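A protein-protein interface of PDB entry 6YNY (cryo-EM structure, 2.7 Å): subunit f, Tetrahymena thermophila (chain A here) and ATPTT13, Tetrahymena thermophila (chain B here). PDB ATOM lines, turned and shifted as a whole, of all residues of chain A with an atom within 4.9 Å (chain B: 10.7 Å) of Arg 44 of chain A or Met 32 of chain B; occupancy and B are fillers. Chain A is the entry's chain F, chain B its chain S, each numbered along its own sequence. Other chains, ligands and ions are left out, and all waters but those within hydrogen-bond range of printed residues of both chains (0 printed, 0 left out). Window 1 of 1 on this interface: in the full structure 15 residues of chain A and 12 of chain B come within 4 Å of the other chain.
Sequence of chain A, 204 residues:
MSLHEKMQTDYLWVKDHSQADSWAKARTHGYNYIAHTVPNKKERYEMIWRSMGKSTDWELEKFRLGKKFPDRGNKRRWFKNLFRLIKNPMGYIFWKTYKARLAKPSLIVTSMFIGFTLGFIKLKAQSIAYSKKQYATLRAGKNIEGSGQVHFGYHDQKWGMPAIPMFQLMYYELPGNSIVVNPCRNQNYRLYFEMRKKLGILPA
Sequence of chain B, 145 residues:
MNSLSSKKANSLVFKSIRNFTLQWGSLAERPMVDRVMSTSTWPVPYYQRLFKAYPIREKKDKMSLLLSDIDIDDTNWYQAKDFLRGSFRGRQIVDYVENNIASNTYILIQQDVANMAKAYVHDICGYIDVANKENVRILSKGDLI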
ATOM      1  N   ALA A  35      21.088  10.370  25.244  1.00  0.00           N
ATOM      2  CA  ALA A  35      22.323  10.763  24.588  1.00  0.00           C
ATOM      3  C   ALA A  35      22.325  10.215  23.168  1.00  0.00           C
ATOM      4  O   ALA A  35      22.132   9.014  22.961  1.00  0.00           O
ATOM      5  CB  ALA A  35      23.534  10.250  25.364  1.00  0.00           C
ATOM      6  N   VAL A  38      27.032   9.751  21.556  1.00  0.00           N
ATOM      7  CA  VAL A  38      28.108   9.019  22.215  1.00  0.00           C
ATOM      8  C   VAL A  38      28.350   7.711  21.475  1.00  0.00           C
ATOM      9  O   VAL A  38      27.428   7.177  20.843  1.00  0.00           O
ATOM     10  CB  VAL A  38      27.785   8.777  23.698  1.00  0.00           C
ATOM     11  CG1 VAL A  38      27.702  10.096  24.434  1.00  0.00           C
ATOM     12  CG2 VAL A  38      26.495   8.004  23.849  1.00  0.00           C
ATOM     13  N   ASN A  40      28.682   4.745  22.598  1.00  0.00           N
ATOM     14  CA  ASN A  40      27.873   3.686  23.186  1.00  0.00           C
ATOM     15  C   ASN A  40      26.386   3.986  23.096  1.00  0.00           C
ATOM     16  O   ASN A  40      25.607   3.534  23.943  1.00  0.00           O
ATOM     17  CB  ASN A  40      28.284   3.459  24.638  1.00  0.00           C
ATOM     18  CG  ASN A  40      28.178   4.707  25.473  1.00  0.00           C
ATOM     19  OD1 ASN A  40      28.373   5.817  24.983  1.00  0.00           O
ATOM     20  ND2 ASN A  40      27.865   4.534  26.743  1.00  0.00           N
ATOM     21  N   LYS A  41      25.977   4.735  22.073  1.00  0.00           N
ATOM     22  CA  LYS A  41      24.579   5.111  21.904  1.00  0.00           C
ATOM     23  C   LYS A  41      23.663   3.897  21.938  1.00  0.00           C
ATOM     24  O   LYS A  41      22.698   3.849  22.708  1.00  0.00           O
ATOM     25  CB  LYS A  41      24.428   5.863  20.583  1.00  0.00           C
ATOM     26  CG  LYS A  41      23.025   6.177  20.155  1.00  0.00           C
ATOM     27  CD  LYS A  41      23.047   6.770  18.765  1.00  0.00           C
ATOM     28  CE  LYS A  41      21.728   7.407  18.400  1.00  0.00           C
ATOM     29  NZ  LYS A  41      21.815   8.159  17.123  1.00  0.00           N
ATOM     30  N   LYS A  42      23.951   2.903  21.101  1.00  0.00           N
ATOM     31  CA  LYS A  42      23.049   1.768  20.966  1.00  0.00           C
ATOM     32  C   LYS A  42      23.048   0.891  22.208  1.00  0.00           C
ATOM     33  O   LYS A  42      22.038   0.246  22.505  1.00  0.00           O
ATOM     34  CB  LYS A  42      23.431   0.957  19.735  1.00  0.00           C
ATOM     35  CG  LYS A  42      23.349   1.759  18.462  1.00  0.00           C
ATOM     36  CD  LYS A  42      23.619   0.914  17.246  1.00  0.00           C
ATOM     37  CE  LYS A  42      23.609   1.747  15.988  1.00  0.00           C
ATOM     38  NZ  LYS A  42      24.698   2.756  15.985  1.00  0.00           N
ATOM     39  N   GLU A  43      24.156   0.855  22.943  1.00  0.00           N
ATOM     40  CA  GLU A  43      24.168   0.126  24.202  1.00  0.00           C
ATOM     41  C   GLU A  43      23.285   0.803  25.238  1.00  0.00           C
ATOM     42  O   GLU A  43      22.748   0.133  26.125  1.00  0.00           O
ATOM     43  CB  GLU A  43      25.595  -0.002  24.725  1.00  0.00           C
ATOM     44  CG  GLU A  43      26.532  -0.727  23.788  1.00  0.00           C
ATOM     45  CD  GLU A  43      27.118   0.175  22.723  1.00  0.00           C
ATOM     46  OE1 GLU A  43      28.329   0.461  22.784  1.00  0.00           O
ATOM     47  OE2 GLU A  43      26.366   0.605  21.828  1.00  0.00           O
ATOM     48  N   ARG A  44      23.116   2.120  25.137  1.00  0.00           N
ATOM     49  CA  ARG A  44      22.225   2.822  26.050  1.00  0.00           C
ATOM     50  C   ARG A  44      20.766   2.516  25.733  1.00  0.00           C
ATOM     51  O   ARG A  44      19.968   2.264  26.643  1.00  0.00           O
ATOM     52  CB  ARG A  44      22.481   4.326  25.979  1.00  0.00           C
ATOM     53  CG  ARG A  44      23.948   4.730  26.037  1.00  0.00           C
ATOM     54  CD  ARG A  44      24.325   5.415  27.318  1.00  0.00           C
ATOM     55  NE  ARG A  44      23.471   6.553  27.614  1.00  0.00           N
ATOM     56  CZ  ARG A  44      23.563   7.275  28.724  1.00  0.00           C
ATOM     57  NH1 ARG A  44      22.743   8.293  28.917  1.00  0.00           N
ATOM     58  NH2 ARG A  44      24.474   6.978  29.636  1.00  0.00           N
ATOM     59  N   TYR A  45      20.399   2.529  24.450  1.00  0.00           N
ATOM     60  CA  TYR A  45      19.036   2.181  24.067  1.00  0.00           C
ATOM     61  C   TYR A  45      18.687   0.762  24.496  1.00  0.00           C
ATOM     62  O   TYR A  45      17.542   0.482  24.865  1.00  0.00           O
ATOM     63  CB  TYR A  45      18.855   2.340  22.559  1.00  0.00           C
ATOM     64  CG  TYR A  45      18.500   3.737  22.111  1.00  0.00           C
ATOM     65  CD1 TYR A  45      17.190   4.185  22.150  1.00  0.00           C
ATOM     66  CD2 TYR A  45      19.468   4.603  21.635  1.00  0.00           C
ATOM     67  CE1 TYR A  45      16.860   5.457  21.738  1.00  0.00           C
ATOM     68  CE2 TYR A  45      19.145   5.875  21.221  1.00  0.00           C
ATOM     69  CZ  TYR A  45      17.840   6.296  21.274  1.00  0.00           C
ATOM     70  OH  TYR A  45      17.514   7.564  20.862  1.00  0.00           O
ATOM     71  N   GLU A  46      19.661  -0.146  24.450  1.00  0.00           N
ATOM     72  CA  GLU A  46      19.401  -1.527  24.837  1.00  0.00           C
ATOM     73  C   GLU A  46      19.100  -1.639  26.325  1.00  0.00           C
ATOM     74  O   GLU A  46      18.258  -2.446  26.733  1.00  0.00           O
ATOM     75  CB  GLU A  46      20.589  -2.406  24.459  1.00  0.00           C
ATOM     76  CG  GLU A  46      20.506  -3.824  24.980  1.00  0.00           C
ATOM     77  CD  GLU A  46      19.230  -4.531  24.570  1.00  0.00           C
ATOM     78  OE1 GLU A  46      18.601  -4.107  23.580  1.00  0.00           O
ATOM     79  OE2 GLU A  46      18.850  -5.511  25.242  1.00  0.00           O
ATOM     80  N   MET A  47      19.782  -0.847  27.149  1.00  0.00           N
ATOM     81  CA  MET A  47      19.503  -0.863  28.579  1.00  0.00           C
ATOM     82  C   MET A  47      18.152  -0.240  28.888  1.00  0.00           C
ATOM     83  O   MET A  47      17.476  -0.665  29.830  1.00  0.00           O
ATOM     84  CB  MET A  47      20.608  -0.141  29.336  1.00  0.00           C
ATOM     85  CG  MET A  47      21.980  -0.752  29.150  1.00  0.00           C
ATOM     86  SD  MET A  47      22.071  -2.492  29.581  1.00  0.00           S
ATOM     87  CE  MET A  47      21.834  -2.388  31.342  1.00  0.00           C
ATOM     88  N   ILE A  48      17.748   0.769  28.118  1.00  0.00           N
ATOM     89  CA  ILE A  48      16.399   1.305  28.254  1.00  0.00           C
ATOM     90  C   ILE A  48      15.378   0.234  27.906  1.00  0.00           C
ATOM     91  O   ILE A  48      14.374   0.057  28.603  1.00  0.00           O
ATOM     92  CB  ILE A  48      16.230   2.552  27.369  1.00  0.00           C
ATOM     93  CG1 ILE A  48      17.238   3.631  27.761  1.00  0.00           C
ATOM     94  CG2 ILE A  48      14.827   3.087  27.480  1.00  0.00           C
ATOM     95  CD1 ILE A  48      17.304   4.791  26.798  1.00  0.00           C
ATOM     96  N   TRP B  24      34.127  11.186  19.392  1.00  0.00           N
ATOM     97  CA  TRP B  24      33.381  10.740  20.555  1.00  0.00           C
ATOM     98  C   TRP B  24      31.964  11.285  20.601  1.00  0.00           C
ATOM     99  O   TRP B  24      31.132  10.743  21.334  1.00  0.00           O
ATOM    100  CB  TRP B  24      34.130  11.128  21.831  1.00  0.00           C
ATOM    101  CG  TRP B  24      35.338  10.286  22.045  1.00  0.00           C
ATOM    102  CD1 TRP B  24      36.575  10.481  21.515  1.00  0.00           C
ATOM    103  CD2 TRP B  24      35.421   9.096  22.832  1.00  0.00           C
ATOM    104  NE1 TRP B  24      37.426   9.491  21.926  1.00  0.00           N
ATOM    105  CE2 TRP B  24      36.742   8.627  22.737  1.00  0.00           C
ATOM    106  CE3 TRP B  24      34.507   8.384  23.609  1.00  0.00           C
ATOM    107  CZ2 TRP B  24      37.171   7.480  23.392  1.00  0.00           C
ATOM    108  CZ3 TRP B  24      34.934   7.250  24.257  1.00  0.00           C
ATOM    109  CH2 TRP B  24      36.254   6.808  24.146  1.00  0.00           C
ATOM    110  N   GLY B  25      31.679  12.349  19.861  1.00  0.00           N
ATOM    111  CA  GLY B  25      30.331  12.860  19.756  1.00  0.00           C
ATOM    112  C   GLY B  25      30.272  14.369  19.745  1.00  0.00           C
ATOM    113  O   GLY B  25      31.236  15.040  19.370  1.00  0.00           O
ATOM    114  N   SER B  26      29.136  14.909  20.163  1.00  0.00           N
ATOM    115  CA  SER B  26      28.950  16.346  20.199  1.00  0.00           C
ATOM    116  C   SER B  26      29.621  16.940  21.430  1.00  0.00           C
ATOM    117  O   SER B  26      29.964  16.242  22.387  1.00  0.00           O
ATOM    118  CB  SER B  26      27.463  16.696  20.190  1.00  0.00           C
ATOM    119  OG  SER B  26      26.764  16.011  21.209  1.00  0.00           O
ATOM    120  N   LEU B  27      29.808  18.257  21.390  1.00  0.00           N
ATOM    121  CA  LEU B  27      30.413  18.945  22.520  1.00  0.00           C
ATOM    122  C   LEU B  27      29.511  18.892  23.743  1.00  0.00           C
ATOM    123  O   LEU B  27      30.003  18.802  24.872  1.00  0.00           O
ATOM    124  CB  LEU B  27      30.716  20.392  22.138  1.00  0.00           C
ATOM    125  CG  LEU B  27      31.389  21.274  23.187  1.00  0.00           C
ATOM    126  CD1 LEU B  27      32.724  20.698  23.596  1.00  0.00           C
ATOM    127  CD2 LEU B  27      31.554  22.678  22.649  1.00  0.00           C
ATOM    128  N   ALA B  28      28.194  18.940  23.538  1.00  0.00           N
ATOM    129  CA  ALA B  28      27.267  18.953  24.660  1.00  0.00           C
ATOM    130  C   ALA B  28      27.278  17.635  25.420  1.00  0.00           C
ATOM    131  O   ALA B  28      27.099  17.626  26.643  1.00  0.00           O
ATOM    132  CB  ALA B  28      25.862  19.267  24.162  1.00  0.00           C
ATOM    133  N   GLU B  29      27.476  16.517  24.725  1.00  0.00           N
ATOM    134  CA  GLU B  29      27.484  15.200  25.341  1.00  0.00           C
ATOM    135  C   GLU B  29      28.887  14.726  25.688  1.00  0.00           C
ATOM    136  O   GLU B  29      29.070  13.553  26.022  1.00  0.00           O
ATOM    137  CB  GLU B  29      26.813  14.187  24.415  1.00  0.00           C
ATOM    138  CG  GLU B  29      25.355  14.482  24.143  1.00  0.00           C
ATOM    139  CD  GLU B  29      24.713  13.469  23.219  1.00  0.00           C
ATOM    140  OE1 GLU B  29      25.332  12.416  22.965  1.00  0.00           O
ATOM    141  OE2 GLU B  29      23.590  13.730  22.743  1.00  0.00           O
ATOM    142  N   ARG B  30      29.877  15.611  25.624  1.00  0.00           N
ATOM    143  CA  ARG B  30      31.243  15.212  25.941  1.00  0.00           C
ATOM    144  C   ARG B  30      31.408  14.682  27.359  1.00  0.00           C
ATOM    145  O   ARG B  30      32.126  13.682  27.529  1.00  0.00           O
ATOM    146  CB  ARG B  30      32.189  16.391  25.701  1.00  0.00           C
ATOM    147  CG  ARG B  30      33.644  16.034  25.898  1.00  0.00           C
ATOM    148  CD  ARG B  30      34.570  17.045  25.273  1.00  0.00           C
ATOM    149  NE  ARG B  30      34.691  18.255  26.074  1.00  0.00           N
ATOM    150  CZ  ARG B  30      35.347  19.339  25.683  1.00  0.00           C
ATOM    151  NH1 ARG B  30      35.937  19.368  24.497  1.00  0.00           N
ATOM    152  NH2 ARG B  30      35.412  20.396  26.478  1.00  0.00           N
ATOM    153  N   PRO B  31      30.802  15.269  28.397  1.00  0.00           N
ATOM    154  CA  PRO B  31      31.012  14.740  29.751  1.00  0.00           C
ATOM    155  C   PRO B  31      30.310  13.416  30.008  1.00  0.00           C
ATOM    156  O   PRO B  31      30.307  12.916  31.136  1.00  0.00           O
ATOM    157  CB  PRO B  31      30.454  15.852  30.646  1.00  0.00           C
ATOM    158  CG  PRO B  31      29.482  16.559  29.816  1.00  0.00           C
ATOM    159  CD  PRO B  31      29.898  16.429  28.396  1.00  0.00           C
ATOM    160  N   MET B  32      29.720  12.836  28.968  1.00  0.00           N
ATOM    161  CA  MET B  32      28.989  11.586  29.106  1.00  0.00           C
ATOM    162  C   MET B  32      29.877  10.360  28.971  1.00  0.00           C
ATOM    163  O   MET B  32      29.586   9.323  29.575  1.00  0.00           O
ATOM    164  CB  MET B  32      27.893  11.520  28.052  1.00  0.00           C
ATOM    165  CG  MET B  32      26.609  10.950  28.549  1.00  0.00           C
ATOM    166  SD  MET B  32      25.744  12.102  29.614  1.00  0.00           S
ATOM    167  CE  MET B  32      24.194  11.242  29.733  1.00  0.00           C
ATOM    168  N   VAL B  33      30.953  10.457  28.186  1.00  0.00           N
ATOM    169  CA  VAL B  33      31.742   9.287  27.810  1.00  0.00           C
ATOM    170  C   VAL B  33      32.769   8.885  28.855  1.00  0.00           C
ATOM    171  O   VAL B  33      33.552   7.958  28.611  1.00  0.00           O
ATOM    172  CB  VAL B  33      32.460   9.552  26.472  1.00  0.00           C
ATOM    173  CG1 VAL B  33      31.467   9.978  25.423  1.00  0.00           C
ATOM    174  CG2 VAL B  33      33.537  10.606  26.646  1.00  0.00           C
ATOM    175  N   ASP B  34      32.797   9.548  30.007  1.00  0.00           N
ATOM    176  CA  ASP B  34      33.854   9.335  30.986  1.00  0.00           C
ATOM    177  C   ASP B  34      33.522   8.266  32.015  1.00  0.00           C
ATOM    178  O   ASP B  34      34.422   7.549  32.465  1.00  0.00           O
ATOM    179  CB  ASP B  34      34.166  10.648  31.700  1.00  0.00           C
ATOM    180  CG  ASP B  34      34.725  11.694  30.764  1.00  0.00           C
ATOM    181  OD1 ASP B  34      33.946  12.248  29.959  1.00  0.00           O
ATOM    182  OD2 ASP B  34      35.943  11.957  30.824  1.00  0.00           O
ATOM    183  N   ARG B  35      32.258   8.146  32.399  1.00  0.00           N
ATOM    184  CA  ARG B  35      31.881   7.252  33.483  1.00  0.00           C
ATOM    185  C   ARG B  35      32.071   5.795  33.083  1.00  0.00           C
ATOM    186  O   ARG B  35      31.712   5.383  31.977  1.00  0.00           O
ATOM    187  CB  ARG B  35      30.429   7.492  33.877  1.00  0.00           C
ATOM    188  CG  ARG B  35      30.010   6.855  35.184  1.00  0.00           C
ATOM    189  CD  ARG B  35      30.535   7.620  36.375  1.00  0.00           C
ATOM    190  NE  ARG B  35      29.805   7.286  37.592  1.00  0.00           N
ATOM    191  CZ  ARG B  35      30.213   6.421  38.511  1.00  0.00           C
ATOM    192  NH1 ARG B  35      31.359   5.771  38.377  1.00  0.00           N
ATOM    193  NH2 ARG B  35      29.456   6.201  39.571  1.00  0.00           N
ATOM    194  N   VAL B  36      32.625   5.010  34.004  1.00  0.00           N
ATOM    195  CA  VAL B  36      32.778   3.571  33.833  1.00  0.00           C
ATOM    196  C   VAL B  36      32.360   2.932  35.149  1.00  0.00           C
ATOM    197  O   VAL B  36      33.067   3.052  36.155  1.00  0.00           O
ATOM    198  CB  VAL B  36      34.210   3.168  33.459  1.00  0.00           C
ATOM    199  CG1 VAL B  36      34.345   1.667  33.405  1.00  0.00           C
ATOM    200  CG2 VAL B  36      34.590   3.766  32.118  1.00  0.00           C
ATOM    201  N   MET B  37      31.217   2.254  35.143  1.00  0.00           N
ATOM    202  CA  MET B  37      30.614   1.722  36.355  1.00  0.00           C
ATOM    203  C   MET B  37      31.035   0.278  36.581  1.00  0.00           C
ATOM    204  O   MET B  37      31.198  -0.494  35.633  1.00  0.00           O
ATOM    205  CB  MET B  37      29.088   1.808  36.272  1.00  0.00           C
ATOM    206  CG  MET B  37      28.537   3.215  36.362  1.00  0.00           C
ATOM    207  SD  MET B  37      28.461   3.837  38.046  1.00  0.00           S
ATOM    208  CE  MET B  37      27.105   2.867  38.681  1.00  0.00           C
ATOM    209  N   THR B  41      23.806  -1.132  37.041  1.00  0.00           N
ATOM    210  CA  THR B  41      22.709  -0.303  37.509  1.00  0.00           C
ATOM    211  C   THR B  41      22.364   0.698  36.420  1.00  0.00           C
ATOM    212  O   THR B  41      23.252   1.282  35.797  1.00  0.00           O
ATOM    213  CB  THR B  41      23.061   0.426  38.806  1.00  0.00           C
ATOM    214  OG1 THR B  41      21.885   1.050  39.338  1.00  0.00           O
ATOM    215  CG2 THR B  41      24.106   1.483  38.556  1.00  0.00           C
ATOM    216  N   TRP B  42      21.068   0.878  36.185  1.00  0.00           N
ATOM    217  CA  TRP B  42      20.595   1.738  35.129  1.00  0.00           C
ATOM    218  C   TRP B  42      19.389   2.530  35.613  1.00  0.00           C
ATOM    219  O   TRP B  42      18.493   1.958  36.250  1.00  0.00           O
ATOM    220  CB  TRP B  42      20.220   0.930  33.881  1.00  0.00           C
ATOM    221  CG  TRP B  42      19.653   1.769  32.802  1.00  0.00           C
ATOM    222  CD1 TRP B  42      18.338   2.016  32.566  1.00  0.00           C
ATOM    223  CD2 TRP B  42      20.382   2.491  31.810  1.00  0.00           C
ATOM    224  NE1 TRP B  42      18.199   2.846  31.489  1.00  0.00           N
ATOM    225  CE2 TRP B  42      19.442   3.153  31.005  1.00  0.00           C
ATOM    226  CE3 TRP B  42      21.739   2.643  31.525  1.00  0.00           C
ATOM    227  CZ2 TRP B  42      19.814   3.951  29.935  1.00  0.00           C
ATOM    228  CZ3 TRP B  42      22.105   3.433  30.465  1.00  0.00           C
ATOM    229  CH2 TRP B  42      21.150   4.078  29.681  1.00  0.00           C
ATOM    230  N   PRO B  43      19.332   3.840  35.332  1.00  0.00           N
ATOM    231  CA  PRO B  43      20.337   4.638  34.628  1.00  0.00           C
ATOM    232  C   PRO B  43      21.580   4.893  35.470  1.00  0.00           C
ATOM    233  O   PRO B  43      21.545   4.705  36.683  1.00  0.00           O
ATOM    234  CB  PRO B  43      19.603   5.941  34.326  1.00  0.00           C
ATOM    235  CG  PRO B  43      18.177   5.643  34.496  1.00  0.00           C
ATOM    236  CD  PRO B  43      18.100   4.608  35.546  1.00  0.00           C
ATOM    237  N   VAL B  44      22.657   5.317  34.830  1.00  0.00           N
ATOM    238  CA  VAL B  44      23.954   5.497  35.475  1.00  0.00           C
ATOM    239  C   VAL B  44      24.225   6.990  35.600  1.00  0.00           C
ATOM    240  O   VAL B  44      24.082   7.716  34.612  1.00  0.00           O
ATOM    241  CB  VAL B  44      25.089   4.809  34.690  1.00  0.00           C
ATOM    242  CG1 VAL B  44      24.854   3.322  34.607  1.00  0.00           C
ATOM    243  CG2 VAL B  44      25.213   5.384  33.306  1.00  0.00           C
ATOM    244  N   PRO B  45      24.593   7.486  36.779  1.00  0.00           N
ATOM    245  CA  PRO B  45      25.043   8.877  36.879  1.00  0.00           C
ATOM    246  C   PRO B  45      26.284   9.115  36.035  1.00  0.00           C
ATOM    247  O   PRO B  45      27.225   8.321  36.042  1.00  0.00           O
ATOM    248  CB  PRO B  45      25.330   9.046  38.371  1.00  0.00           C
ATOM    249  CG  PRO B  45      24.498   8.039  39.029  1.00  0.00           C
ATOM    250  CD  PRO B  45      24.438   6.872  38.107  1.00  0.00           C
ATOM    251  N   TYR B  46      26.282  10.232  35.308  1.00  0.00           N
ATOM    252  CA  TYR B  46      27.332  10.487  34.333  1.00  0.00           C
ATOM    253  C   TYR B  46      28.611  11.001  34.976  1.00  0.00           C
ATOM    254  O   TYR B  46      29.704  10.698  34.489  1.00  0.00           O
ATOM    255  CB  TYR B  46      26.843  11.488  33.286  1.00  0.00           C
ATOM    256  CG  TYR B  46      26.868  12.929  33.727  1.00  0.00           C
ATOM    257  CD1 TYR B  46      27.957  13.736  33.449  1.00  0.00           C
ATOM    258  CD2 TYR B  46      25.804  13.488  34.408  1.00  0.00           C
ATOM    259  CE1 TYR B  46      27.989  15.046  33.846  1.00  0.00           C
ATOM    260  CE2 TYR B  46      25.826  14.800  34.805  1.00  0.00           C
ATOM    261  CZ  TYR B  46      26.924  15.578  34.518  1.00  0.00           C
ATOM    262  OH  TYR B  46      26.971  16.895  34.908  1.00  0.00           O
ATOM    263  N   TYR B  47      28.501  11.765  36.056  1.00  0.00           N
ATOM    264  CA  TYR B  47      29.651  12.489  36.572  1.00  0.00           C
ATOM    265  C   TYR B  47      30.752  11.531  36.995  1.00  0.00           C
ATOM    266  O   TYR B  47      30.517  10.587  37.753  1.00  0.00           O
ATOM    267  CB  TYR B  47      29.239  13.368  37.745  1.00  0.00           C
ATOM    268  CG  TYR B  47      30.256  14.425  38.075  1.00  0.00           C
ATOM    269  CD1 TYR B  47      30.289  15.616  37.378  1.00  0.00           C
ATOM    270  CD2 TYR B  47      31.190  14.228  39.075  1.00  0.00           C
ATOM    271  CE1 TYR B  47      31.218  16.581  37.668  1.00  0.00           C
ATOM    272  CE2 TYR B  47      32.122  15.188  39.371  1.00  0.00           C
ATOM    273  CZ  TYR B  47      32.133  16.363  38.663  1.00  0.00           C
ATOM    274  OH  TYR B  47      33.062  17.328  38.955  1.00  0.00           O
ATOM    275  N   GLN B  48      31.958  11.782  36.501  1.00  0.00           N
ATOM    276  CA  GLN B  48      33.141  11.035  36.894  1.00  0.00           C
ATOM    277  C   GLN B  48      33.931  11.870  37.888  1.00  0.00           C
ATOM    278  O   GLN B  48      34.350  12.990  37.575  1.00  0.00           O
ATOM    279  CB  GLN B  48      33.993  10.682  35.676  1.00  0.00           C
ATOM    280  CG  GLN B  48      35.305   9.990  36.002  1.00  0.00           C
ATOM    281  CD  GLN B  48      35.125   8.750  36.844  1.00  0.00           C
ATOM    282  OE1 GLN B  48      34.171   7.996  36.663  1.00  0.00           O
ATOM    283  NE2 GLN B  48      36.040   8.535  37.787  1.00  0.00           N
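The backbone NH of Val 38 of chain A sits at hydrogen-bond distance from the side-chain carboxylate of Glu 29 of chain B (3.5 Å).
Among the printed residues, merely in contact across the chains: Ile 48 of chain A with Trp 42 of chain B (3.4 Å), Arg 44 of chain A with Met 32 of chain B (3.4 Å), Val 38 of chain A with Trp 24 of chain B (3.6 Å), Met 47 of chain A with Trp 42 of chain B (3.6 Å), Ala 35 of chain A with Glu 29 of chain B (3.7 Å), Arg 44 of chain A with Trp 42 of chain B (3.7 Å), Val 38 of chain A with Met 32 of chain B (3.9 Å) and Val 38 of chain A with Val 33 of chain B (3.9 Å).
Of chain B, only Met 32 (3.4 Å) and Trp 42 (3.7 Å) come within 4 Å of Arg 44 of chain A.
Met 32 of chain B touches just these residues of chain A: Val 38 and Arg 44.
No residue of chain B comes within 4 Å of Asn 40 of chain A.
No residue of chain B comes within 4 Å of Glu 43 of chain A.
Printed residues of chain A within 4 Å of Trp 42 of chain B: Arg 44, Met 47 and Ile 48.
Printed residues of chain B within 4 Å of Met 47 of chain A: Trp 42 (3.6 Å).
Printed residues of chain B within 4 Å of Val 38 of chain A: Trp 24, Glu 29, Met 32 and Val 33.
Printed residues of chain A within 4 Å of Glu 29 of chain B: Ala 35 and Val 38.
Printed residues of chain A within 4 Å of Trp 24 of chain B: Val 38.
Lys 41 of chain A touches none of the printed residues of chain B.
Pro 31 of chain B touches none of the printed residues of chain A.
The nearest residue of chain A that does not touch Met 32 of chain B is Ala 35 of chain A (4.5 Å).
Of the 11 printed residues of chain A, 5 touch a printed residue of chain B.
Printed residues of chain A that touch a printed residue of chain B: Ala 35, Val 38, Arg 44, Met 47 and Ile 48.
Along chain A the printed residues that touch a printed residue of chain B span positions 35 to 48.
Of the 22 printed residues of chain B, 5 touch a printed residue of chain A.
Among the printed residues, no Asp or Glu carboxylate lies within 4 Å of a Lys or Arg side-chain nitrogen of the other chain.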
